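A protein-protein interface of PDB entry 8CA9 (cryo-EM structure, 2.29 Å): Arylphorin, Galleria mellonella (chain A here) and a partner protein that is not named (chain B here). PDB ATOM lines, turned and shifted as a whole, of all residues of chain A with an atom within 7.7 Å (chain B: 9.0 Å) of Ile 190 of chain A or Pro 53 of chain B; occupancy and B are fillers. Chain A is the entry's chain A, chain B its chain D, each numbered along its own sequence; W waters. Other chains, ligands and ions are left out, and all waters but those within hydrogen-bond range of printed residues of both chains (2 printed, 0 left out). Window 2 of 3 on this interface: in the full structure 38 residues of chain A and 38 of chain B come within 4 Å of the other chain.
NE2 of Gln 185 of chain A is in hydrogen-bond range of O of Gly 187 of chain A (3.3 Å).
The backbone carbonyl oxygen (O) of Gln 50 of chain B is in hydrogen-bond range of the side-chain amide nitrogen (ND2) of Asn 47 of chain B (3.3 Å).
The backbone carbonyl oxygen of Gln 50 of chain B sits at hydrogen-bond distance from the guanidinium group of Arg 132 of chain B (3.1 Å).
O of Arg 132 of chain B is in hydrogen-bond range of NZ of Lys 93 of chain B, at 3.4 Å.
The side-chain amide oxygen (OE1) of Gln 185 of chain A is in hydrogen-bond range of the side-chain amide nitrogen (NE2) of Gln 50 of chain B (2.8 Å).
Among the printed residues, merely in contact across the chains: Ile 189 of chain A with Glu 488 of chain B (3.3 Å), Ile 190 of chain A with Pro 53 of chain B (3.7 Å), Tyr 197 of chain A with Lys 93 of chain B (3.7 Å) and Ile 190 of chain A with Val 51 of chain B (3.9 Å).
Water W2 bridges the backbone carbonyl oxygen of Gln 185 of chain A (2.7 Å) and the backbone NH of Glu 488 of chain B (3.1 Å).
Water W1 lies within hydrogen-bond range of the side-chain hydroxyl (OH) of Tyr 197 of chain A (3.3 Å) and the backbone NH (N) of Lys 93 of chain B (3.3 Å).
Of the printed residues of chain B, Gln 185 of chain A touches Gln 50.
Of chain B, only Val 51 (3.9 Å) and Pro 53 (3.7 Å) come within 4 Å of Ile 190 of chain A.
Of the printed residues of chain A, Gln 50 of chain B touches Gln 185.
Printed residues of chain A within 4 Å of Val 51 of chain B: Ile 190 (3.9 Å).
Of the printed residues of chain A, Pro 53 of chain B touches Ile 190 (3.7 Å).
Asp 54 of chain B touches none of the printed residues of chain A.
Of the printed residues of chain A, Glu 488 of chain B touches Ile 189.
Of the 11 printed residues of chain A, 4 touch a printed residue of chain B.
Of the 19 printed residues of chain B, 5 touch a printed residue of chain A.
Among the printed residues, 5 pairs touch across the chains.
Among the printed residues, no Asp or Glu carboxylate lies within 4 Å of a Lys or Arg side-chain nitrogen of the other chain.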
ATOM      1  N   GLN A 185      14.062   8.857  -2.785  1.00  0.00           N
ATOM      2  CA  GLN A 185      13.314   9.475  -3.870  1.00  0.00           C
ATOM      3  C   GLN A 185      11.902   9.876  -3.468  1.00  0.00           C
ATOM      4  O   GLN A 185      11.245  10.602  -4.222  1.00  0.00           O
ATOM      5  CB  GLN A 185      13.244   8.524  -5.071  1.00  0.00           C
ATOM      6  CG  GLN A 185      14.598   8.157  -5.659  1.00  0.00           C
ATOM      7  CD  GLN A 185      14.500   7.279  -6.899  1.00  0.00           C
ATOM      8  OE1 GLN A 185      15.426   7.237  -7.709  1.00  0.00           O
ATOM      9  NE2 GLN A 185      13.384   6.573  -7.052  1.00  0.00           N
ATOM     10  N   GLY A 187       9.286   8.084  -3.488  1.00  0.00           N
ATOM     11  CA  GLY A 187       8.416   7.491  -4.475  1.00  0.00           C
ATOM     12  C   GLY A 187       9.207   7.027  -5.675  1.00  0.00           C
ATOM     13  O   GLY A 187      10.429   6.850  -5.610  1.00  0.00           O
ATOM     14  N   LEU A 188       8.498   6.830  -6.782  1.00  0.00           N
ATOM     15  CA  LEU A 188       9.086   6.382  -8.037  1.00  0.00           C
ATOM     16  C   LEU A 188       9.090   7.534  -9.032  1.00  0.00           C
ATOM     17  O   LEU A 188       8.051   8.162  -9.264  1.00  0.00           O
ATOM     18  CB  LEU A 188       8.309   5.196  -8.609  1.00  0.00           C
ATOM     19  CG  LEU A 188       8.343   3.904  -7.792  1.00  0.00           C
ATOM     20  CD1 LEU A 188       7.211   2.982  -8.211  1.00  0.00           C
ATOM     21  CD2 LEU A 188       9.685   3.207  -7.950  1.00  0.00           C
ATOM     22  N   ILE A 189      10.257   7.807  -9.616  1.00  0.00           N
ATOM     23  CA  ILE A 189      10.347   8.848 -10.634  1.00  0.00           C
ATOM     24  C   ILE A 189       9.538   8.456 -11.862  1.00  0.00           C
ATOM     25  O   ILE A 189       8.825   9.281 -12.445  1.00  0.00           O
ATOM     26  CB  ILE A 189      11.820   9.118 -10.992  1.00  0.00           C
ATOM     27  CG1 ILE A 189      12.647   9.384  -9.728  1.00  0.00           C
ATOM     28  CG2 ILE A 189      11.929  10.290 -11.952  1.00  0.00           C
ATOM     29  CD1 ILE A 189      12.108  10.497  -8.854  1.00  0.00           C
ATOM     30  N   ILE A 190       9.634   7.194 -12.271  1.00  0.00           N
ATOM     31  CA  ILE A 190       8.864   6.663 -13.393  1.00  0.00           C
ATOM     32  C   ILE A 190       8.090   5.455 -12.879  1.00  0.00           C
ATOM     33  O   ILE A 190       8.613   4.332 -12.901  1.00  0.00           O
ATOM     34  CB  ILE A 190       9.773   6.295 -14.577  1.00  0.00           C
ATOM     35  CG1 ILE A 190      10.724   7.453 -14.892  1.00  0.00           C
ATOM     36  CG2 ILE A 190       8.933   5.953 -15.801  1.00  0.00           C
ATOM     37  CD1 ILE A 190      11.674   7.180 -16.038  1.00  0.00           C
ATOM     38  N   PRO A 191       6.853   5.632 -12.401  1.00  0.00           N
ATOM     39  CA  PRO A 191       6.159   4.503 -11.754  1.00  0.00           C
ATOM     40  C   PRO A 191       5.971   3.301 -12.661  1.00  0.00           C
ATOM     41  O   PRO A 191       5.987   2.160 -12.179  1.00  0.00           O
ATOM     42  CB  PRO A 191       4.816   5.117 -11.332  1.00  0.00           C
ATOM     43  CG  PRO A 191       4.626   6.289 -12.225  1.00  0.00           C
ATOM     44  CD  PRO A 191       5.995   6.825 -12.502  1.00  0.00           C
ATOM     45  N   GLU A 192       5.796   3.521 -13.965  1.00  0.00           N
ATOM     46  CA  GLU A 192       5.509   2.416 -14.874  1.00  0.00           C
ATOM     47  C   GLU A 192       6.618   1.374 -14.897  1.00  0.00           C
ATOM     48  O   GLU A 192       6.348   0.207 -15.203  1.00  0.00           O
ATOM     49  CB  GLU A 192       5.272   2.951 -16.287  1.00  0.00           C
ATOM     50  CG  GLU A 192       3.926   3.639 -16.468  1.00  0.00           C
ATOM     51  CD  GLU A 192       3.845   4.972 -15.750  1.00  0.00           C
ATOM     52  OE1 GLU A 192       4.905   5.509 -15.368  1.00  0.00           O
ATOM     53  OE2 GLU A 192       2.719   5.483 -15.564  1.00  0.00           O
ATOM     54  N   GLN A 193       7.852   1.759 -14.579  1.00  0.00           N
ATOM     55  CA  GLN A 193       8.981   0.841 -14.629  1.00  0.00           C
ATOM     56  C   GLN A 193       9.238   0.127 -13.306  1.00  0.00           C
ATOM     57  O   GLN A 193      10.144  -0.710 -13.240  1.00  0.00           O
ATOM     58  CB  GLN A 193      10.245   1.594 -15.059  1.00  0.00           C
ATOM     59  CG  GLN A 193      10.063   2.400 -16.337  1.00  0.00           C
ATOM     60  CD  GLN A 193      11.375   2.894 -16.915  1.00  0.00           C
ATOM     61  OE1 GLN A 193      11.623   2.767 -18.115  1.00  0.00           O
ATOM     62  NE2 GLN A 193      12.220   3.464 -16.066  1.00  0.00           N
ATOM     63  N   GLY A 194       8.468   0.428 -12.264  1.00  0.00           N
ATOM     64  CA  GLY A 194       8.664  -0.175 -10.966  1.00  0.00           C
ATOM     65  C   GLY A 194       8.450  -1.676 -10.947  1.00  0.00           C
ATOM     66  O   GLY A 194       9.255  -2.427 -10.389  1.00  0.00           O
ATOM     67  N   PRO A 195       7.354  -2.147 -11.550  1.00  0.00           N
ATOM     68  CA  PRO A 195       7.084  -3.594 -11.527  1.00  0.00           C
ATOM     69  C   PRO A 195       8.188  -4.433 -12.146  1.00  0.00           C
ATOM     70  O   PRO A 195       8.421  -5.561 -11.693  1.00  0.00           O
ATOM     71  CB  PRO A 195       5.773  -3.716 -12.318  1.00  0.00           C
ATOM     72  CG  PRO A 195       5.118  -2.395 -12.166  1.00  0.00           C
ATOM     73  CD  PRO A 195       6.225  -1.386 -12.111  1.00  0.00           C
ATOM     74  N   TYR A 197      11.216  -4.182 -11.755  1.00  0.00           N
ATOM     75  CA  TYR A 197      12.286  -4.361 -10.783  1.00  0.00           C
ATOM     76  C   TYR A 197      11.777  -4.892  -9.448  1.00  0.00           C
ATOM     77  O   TYR A 197      12.519  -4.865  -8.459  1.00  0.00           O
ATOM     78  CB  TYR A 197      13.034  -3.042 -10.572  1.00  0.00           C
ATOM     79  CG  TYR A 197      13.575  -2.445 -11.851  1.00  0.00           C
ATOM     80  CD1 TYR A 197      14.733  -2.939 -12.435  1.00  0.00           C
ATOM     81  CD2 TYR A 197      12.928  -1.389 -12.475  1.00  0.00           C
ATOM     82  CE1 TYR A 197      15.230  -2.398 -13.604  1.00  0.00           C
ATOM     83  CE2 TYR A 197      13.416  -0.840 -13.644  1.00  0.00           C
ATOM     84  CZ  TYR A 197      14.569  -1.349 -14.205  1.00  0.00           C
ATOM     85  OH  TYR A 197      15.062  -0.808 -15.370  1.00  0.00           O
ATOM     86  N   ASN B  47      23.335  13.843 -12.514  1.00  0.00           N
ATOM     87  CA  ASN B  47      22.553  12.749 -11.936  1.00  0.00           C
ATOM     88  C   ASN B  47      22.438  11.581 -12.914  1.00  0.00           C
ATOM     89  O   ASN B  47      21.349  11.119 -13.258  1.00  0.00           O
ATOM     90  CB  ASN B  47      21.172  13.238 -11.496  1.00  0.00           C
ATOM     91  CG  ASN B  47      20.330  13.741 -12.653  1.00  0.00           C
ATOM     92  OD1 ASN B  47      20.395  14.915 -13.017  1.00  0.00           O
ATOM     93  ND2 ASN B  47      19.532  12.853 -13.234  1.00  0.00           N
ATOM     94  N   GLN B  50      20.212   8.408 -12.528  1.00  0.00           N
ATOM     95  CA  GLN B  50      18.766   8.479 -12.684  1.00  0.00           C
ATOM     96  C   GLN B  50      18.421   9.061 -14.046  1.00  0.00           C
ATOM     97  O   GLN B  50      19.178   9.854 -14.613  1.00  0.00           O
ATOM     98  CB  GLN B  50      18.126   9.333 -11.582  1.00  0.00           C
ATOM     99  CG  GLN B  50      18.400   8.840 -10.172  1.00  0.00           C
ATOM    100  CD  GLN B  50      17.819   9.757  -9.114  1.00  0.00           C
ATOM    101  OE1 GLN B  50      18.500  10.644  -8.602  1.00  0.00           O
ATOM    102  NE2 GLN B  50      16.552   9.547  -8.780  1.00  0.00           N
ATOM    103  N   VAL B  51      17.263   8.658 -14.565  1.00  0.00           N
ATOM    104  CA  VAL B  51      16.734   9.161 -15.827  1.00  0.00           C
ATOM    105  C   VAL B  51      15.537  10.046 -15.509  1.00  0.00           C
ATOM    106  O   VAL B  51      14.563   9.590 -14.897  1.00  0.00           O
ATOM    107  CB  VAL B  51      16.341   8.017 -16.774  1.00  0.00           C
ATOM    108  CG1 VAL B  51      15.529   8.549 -17.947  1.00  0.00           C
ATOM    109  CG2 VAL B  51      17.581   7.292 -17.271  1.00  0.00           C
ATOM    110  N   ASP B  52      15.610  11.310 -15.926  1.00  0.00           N
ATOM    111  CA  ASP B  52      14.546  12.271 -15.667  1.00  0.00           C
ATOM    112  C   ASP B  52      13.705  12.442 -16.920  1.00  0.00           C
ATOM    113  O   ASP B  52      14.222  12.941 -17.932  1.00  0.00           O
ATOM    114  CB  ASP B  52      15.132  13.611 -15.241  1.00  0.00           C
ATOM    115  CG  ASP B  52      14.069  14.597 -14.798  1.00  0.00           C
ATOM    116  OD1 ASP B  52      12.879  14.222 -14.771  1.00  0.00           O
ATOM    117  OD2 ASP B  52      14.424  15.751 -14.474  1.00  0.00           O
ATOM    118  N   PRO B  53      12.427  12.052 -16.918  1.00  0.00           N
ATOM    119  CA  PRO B  53      11.614  12.222 -18.134  1.00  0.00           C
ATOM    120  C   PRO B  53      11.464  13.667 -18.577  1.00  0.00           C
ATOM    121  O   PRO B  53      11.210  13.908 -19.764  1.00  0.00           O
ATOM    122  CB  PRO B  53      10.259  11.616 -17.739  1.00  0.00           C
ATOM    123  CG  PRO B  53      10.558  10.701 -16.607  1.00  0.00           C
ATOM    124  CD  PRO B  53      11.698  11.323 -15.867  1.00  0.00           C
ATOM    125  N   ASP B  54      11.610  14.633 -17.674  1.00  0.00           N
ATOM    126  CA  ASP B  54      11.405  16.039 -17.999  1.00  0.00           C
ATOM    127  C   ASP B  54      12.624  16.693 -18.638  1.00  0.00           C
ATOM    128  O   ASP B  54      12.538  17.858 -19.042  1.00  0.00           O
ATOM    129  CB  ASP B  54      11.013  16.818 -16.739  1.00  0.00           C
ATOM    130  CG  ASP B  54       9.603  16.506 -16.275  1.00  0.00           C
ATOM    131  OD1 ASP B  54       8.715  16.341 -17.139  1.00  0.00           O
ATOM    132  OD2 ASP B  54       9.386  16.424 -15.047  1.00  0.00           O
ATOM    133  N   ASP B  55      13.748  15.989 -18.738  1.00  0.00           N
ATOM    134  CA  ASP B  55      14.936  16.569 -19.342  1.00  0.00           C
ATOM    135  C   ASP B  55      14.873  16.474 -20.864  1.00  0.00           C
ATOM    136  O   ASP B  55      14.132  15.671 -21.437  1.00  0.00           O
ATOM    137  CB  ASP B  55      16.198  15.879 -18.825  1.00  0.00           C
ATOM    138  CG  ASP B  55      16.637  16.400 -17.469  1.00  0.00           C
ATOM    139  OD1 ASP B  55      16.383  17.587 -17.175  1.00  0.00           O
ATOM    140  OD2 ASP B  55      17.243  15.625 -16.701  1.00  0.00           O
ATOM    141  N   GLU B  56      15.675  17.318 -21.518  1.00  0.00           N
ATOM    142  CA  GLU B  56      15.658  17.388 -22.975  1.00  0.00           C
ATOM    143  C   GLU B  56      16.122  16.080 -23.605  1.00  0.00           C
ATOM    144  O   GLU B  56      15.537  15.620 -24.593  1.00  0.00           O
ATOM    145  CB  GLU B  56      16.530  18.555 -23.443  1.00  0.00           C
ATOM    146  CG  GLU B  56      16.847  18.583 -24.939  1.00  0.00           C
ATOM    147  CD  GLU B  56      15.616  18.730 -25.817  1.00  0.00           C
ATOM    148  OE1 GLU B  56      14.556  18.163 -25.477  1.00  0.00           O
ATOM    149  OE2 GLU B  56      15.708  19.416 -26.857  1.00  0.00           O
ATOM    150  N   TYR B  57      17.171  15.466 -23.053  1.00  0.00           N
ATOM    151  CA  TYR B  57      17.742  14.275 -23.671  1.00  0.00           C
ATOM    152  C   TYR B  57      16.767  13.106 -23.702  1.00  0.00           C
ATOM    153  O   TYR B  57      16.947  12.187 -24.507  1.00  0.00           O
ATOM    154  CB  TYR B  57      19.019  13.860 -22.933  1.00  0.00           C
ATOM    155  CG  TYR B  57      18.794  13.414 -21.504  1.00  0.00           C
ATOM    156  CD1 TYR B  57      18.415  12.110 -21.213  1.00  0.00           C
ATOM    157  CD2 TYR B  57      18.971  14.294 -20.445  1.00  0.00           C
ATOM    158  CE1 TYR B  57      18.210  11.698 -19.910  1.00  0.00           C
ATOM    159  CE2 TYR B  57      18.771  13.890 -19.138  1.00  0.00           C
ATOM    160  CZ  TYR B  57      18.390  12.591 -18.878  1.00  0.00           C
ATOM    161  OH  TYR B  57      18.188  12.184 -17.579  1.00  0.00           O
ATOM    162  N   TYR B  58      15.743  13.115 -22.846  1.00  0.00           N
ATOM    163  CA  TYR B  58      14.860  11.958 -22.739  1.00  0.00           C
ATOM    164  C   TYR B  58      14.104  11.717 -24.040  1.00  0.00           C
ATOM    165  O   TYR B  58      14.048  10.587 -24.538  1.00  0.00           O
ATOM    166  CB  TYR B  58      13.886  12.153 -21.577  1.00  0.00           C
ATOM    167  CG  TYR B  58      13.083  10.918 -21.242  1.00  0.00           C
ATOM    168  CD1 TYR B  58      13.675   9.833 -20.613  1.00  0.00           C
ATOM    169  CD2 TYR B  58      11.730  10.840 -21.546  1.00  0.00           C
ATOM    170  CE1 TYR B  58      12.947   8.702 -20.302  1.00  0.00           C
ATOM    171  CE2 TYR B  58      10.993   9.713 -21.236  1.00  0.00           C
ATOM    172  CZ  TYR B  58      11.606   8.648 -20.614  1.00  0.00           C
ATOM    173  OH  TYR B  58      10.877   7.522 -20.305  1.00  0.00           O
ATOM    174  N   LYS B  59      13.505  12.771 -24.600  1.00  0.00           N
ATOM    175  CA  LYS B  59      12.748  12.610 -25.837  1.00  0.00           C
ATOM    176  C   LYS B  59      13.655  12.175 -26.981  1.00  0.00           C
ATOM    177  O   LYS B  59      13.294  11.295 -27.772  1.00  0.00           O
ATOM    178  CB  LYS B  59      12.035  13.917 -26.186  1.00  0.00           C
ATOM    179  CG  LYS B  59      10.928  13.778 -27.229  1.00  0.00           C
ATOM    180  CD  LYS B  59       9.848  12.777 -26.816  1.00  0.00           C
ATOM    181  CE  LYS B  59       9.293  13.071 -25.427  1.00  0.00           C
ATOM    182  NZ  LYS B  59       8.177  12.157 -25.063  1.00  0.00           N
ATOM    183  N   ILE B  60      14.841  12.779 -27.078  1.00  0.00           N
ATOM    184  CA  ILE B  60      15.773  12.427 -28.146  1.00  0.00           C
ATOM    185  C   ILE B  60      16.162  10.959 -28.040  1.00  0.00           C
ATOM    186  O   ILE B  60      16.179  10.228 -29.037  1.00  0.00           O
ATOM    187  CB  ILE B  60      17.007  13.346 -28.098  1.00  0.00           C
ATOM    188  CG1 ILE B  60      16.592  14.806 -28.296  1.00  0.00           C
ATOM    189  CG2 ILE B  60      18.016  12.937 -29.160  1.00  0.00           C
ATOM    190  CD1 ILE B  60      17.618  15.804 -27.812  1.00  0.00           C
ATOM    191  N   LYS B  62      14.482   8.516 -26.527  1.00  0.00           N
ATOM    192  CA  LYS B  62      13.326   7.663 -26.774  1.00  0.00           C
ATOM    193  C   LYS B  62      12.920   7.641 -28.242  1.00  0.00           C
ATOM    194  O   LYS B  62      12.255   6.692 -28.670  1.00  0.00           O
ATOM    195  CB  LYS B  62      12.143   8.124 -25.921  1.00  0.00           C
ATOM    196  CG  LYS B  62      11.999   7.380 -24.604  1.00  0.00           C
ATOM    197  CD  LYS B  62      11.366   6.014 -24.809  1.00  0.00           C
ATOM    198  CE  LYS B  62      11.455   5.159 -23.555  1.00  0.00           C
ATOM    199  NZ  LYS B  62      10.851   5.828 -22.371  1.00  0.00           N
ATOM    200  N   LYS B  93      19.364  -2.424 -16.147  1.00  0.00           N
ATOM    201  CA  LYS B  93      19.726  -1.246 -15.377  1.00  0.00           C
ATOM    202  C   LYS B  93      19.874  -1.602 -13.899  1.00  0.00           C
ATOM    203  O   LYS B  93      19.469  -2.674 -13.443  1.00  0.00           O
ATOM    204  CB  LYS B  93      18.675  -0.150 -15.548  1.00  0.00           C
ATOM    205  CG  LYS B  93      18.705   0.549 -16.896  1.00  0.00           C
ATOM    206  CD  LYS B  93      17.533   1.509 -17.042  1.00  0.00           C
ATOM    207  CE  LYS B  93      17.643   2.339 -18.310  1.00  0.00           C
ATOM    208  NZ  LYS B  93      18.771   3.307 -18.246  1.00  0.00           N
ATOM    209  N   ARG B 132      21.960   6.695 -22.575  1.00  0.00           N
ATOM    210  CA  ARG B 132      21.518   7.003 -21.220  1.00  0.00           C
ATOM    211  C   ARG B 132      20.064   6.611 -21.005  1.00  0.00           C
ATOM    212  O   ARG B 132      19.715   6.094 -19.938  1.00  0.00           O
ATOM    213  CB  ARG B 132      21.707   8.489 -20.917  1.00  0.00           C
ATOM    214  CG  ARG B 132      21.217   8.885 -19.533  1.00  0.00           C
ATOM    215  CD  ARG B 132      21.706  10.259 -19.114  1.00  0.00           C
ATOM    216  NE  ARG B 132      21.217  10.615 -17.787  1.00  0.00           N
ATOM    217  CZ  ARG B 132      21.565  11.710 -17.124  1.00  0.00           C
ATOM    218  NH1 ARG B 132      22.419  12.584 -17.630  1.00  0.00           N
ATOM    219  NH2 ARG B 132      21.045  11.931 -15.920  1.00  0.00           N
ATOM    220  N   VAL B 133      19.206   6.840 -22.000  1.00  0.00           N
ATOM    221  CA  VAL B 133      17.794   6.513 -21.843  1.00  0.00           C
ATOM    222  C   VAL B 133      17.597   5.005 -21.731  1.00  0.00           C
ATOM    223  O   VAL B 133      16.817   4.532 -20.895  1.00  0.00           O
ATOM    224  CB  VAL B 133      16.982   7.105 -23.010  1.00  0.00           C
ATOM    225  CG1 VAL B 133      15.597   6.487 -23.063  1.00  0.00           C
ATOM    226  CG2 VAL B 133      16.888   8.618 -22.875  1.00  0.00           C
ATOM    227  N   GLU B 488      11.789  13.910  -7.157  1.00  0.00           N
ATOM    228  CA  GLU B 488      11.296  14.620  -8.333  1.00  0.00           C
ATOM    229  C   GLU B 488      11.435  16.127  -8.160  1.00  0.00           C
ATOM    230  O   GLU B 488      11.851  16.832  -9.087  1.00  0.00           O
ATOM    231  CB  GLU B 488       9.838  14.247  -8.598  1.00  0.00           C
ATOM    232  CG  GLU B 488       9.312  14.729  -9.942  1.00  0.00           C
ATOM    233  CD  GLU B 488       9.830  13.900 -11.100  1.00  0.00           C
ATOM    234  OE1 GLU B 488       9.805  12.655 -10.997  1.00  0.00           O
ATOM    235  OE2 GLU B 488      10.269  14.492 -12.109  1.00  0.00           O
ATOM    236  N   LEU B 491      15.081  17.090  -8.589  1.00  0.00           N
ATOM    237  CA  LEU B 491      15.467  17.050  -9.994  1.00  0.00           C
ATOM    238  C   LEU B 491      14.916  18.252 -10.749  1.00  0.00           C
ATOM    239  O   LEU B 491      15.610  18.838 -11.588  1.00  0.00           O
ATOM    240  CB  LEU B 491      14.976  15.749 -10.634  1.00  0.00           C
ATOM    241  CG  LEU B 491      15.575  14.452 -10.089  1.00  0.00           C
ATOM    242  CD1 LEU B 491      14.805  13.246 -10.607  1.00  0.00           C
ATOM    243  CD2 LEU B 491      17.043  14.345 -10.458  1.00  0.00           C
ATOM    244  N   ASP B 492      13.670  18.634 -10.464  1.00  0.00           N
ATOM    245  CA  ASP B 492      13.024  19.703 -11.215  1.00  0.00           C
ATOM    246  C   ASP B 492      13.602  21.076 -10.898  1.00  0.00           C
ATOM    247  O   ASP B 492      13.770  21.892 -11.810  1.00  0.00           O
ATOM    248  CB  ASP B 492      11.522  19.700 -10.935  1.00  0.00           C
ATOM    249  CG  ASP B 492      10.845  18.428 -11.401  1.00  0.00           C
ATOM    250  OD1 ASP B 492      11.537  17.560 -11.973  1.00  0.00           O
ATOM    251  OD2 ASP B 492       9.620  18.294 -11.195  1.00  0.00           O
HETATM  252  O   HOH W   1      16.308  -3.112 -17.298  1.00  0.00           O
HETATM  253  O   HOH W   2       9.684  12.225  -5.655  1.00  0.00           O
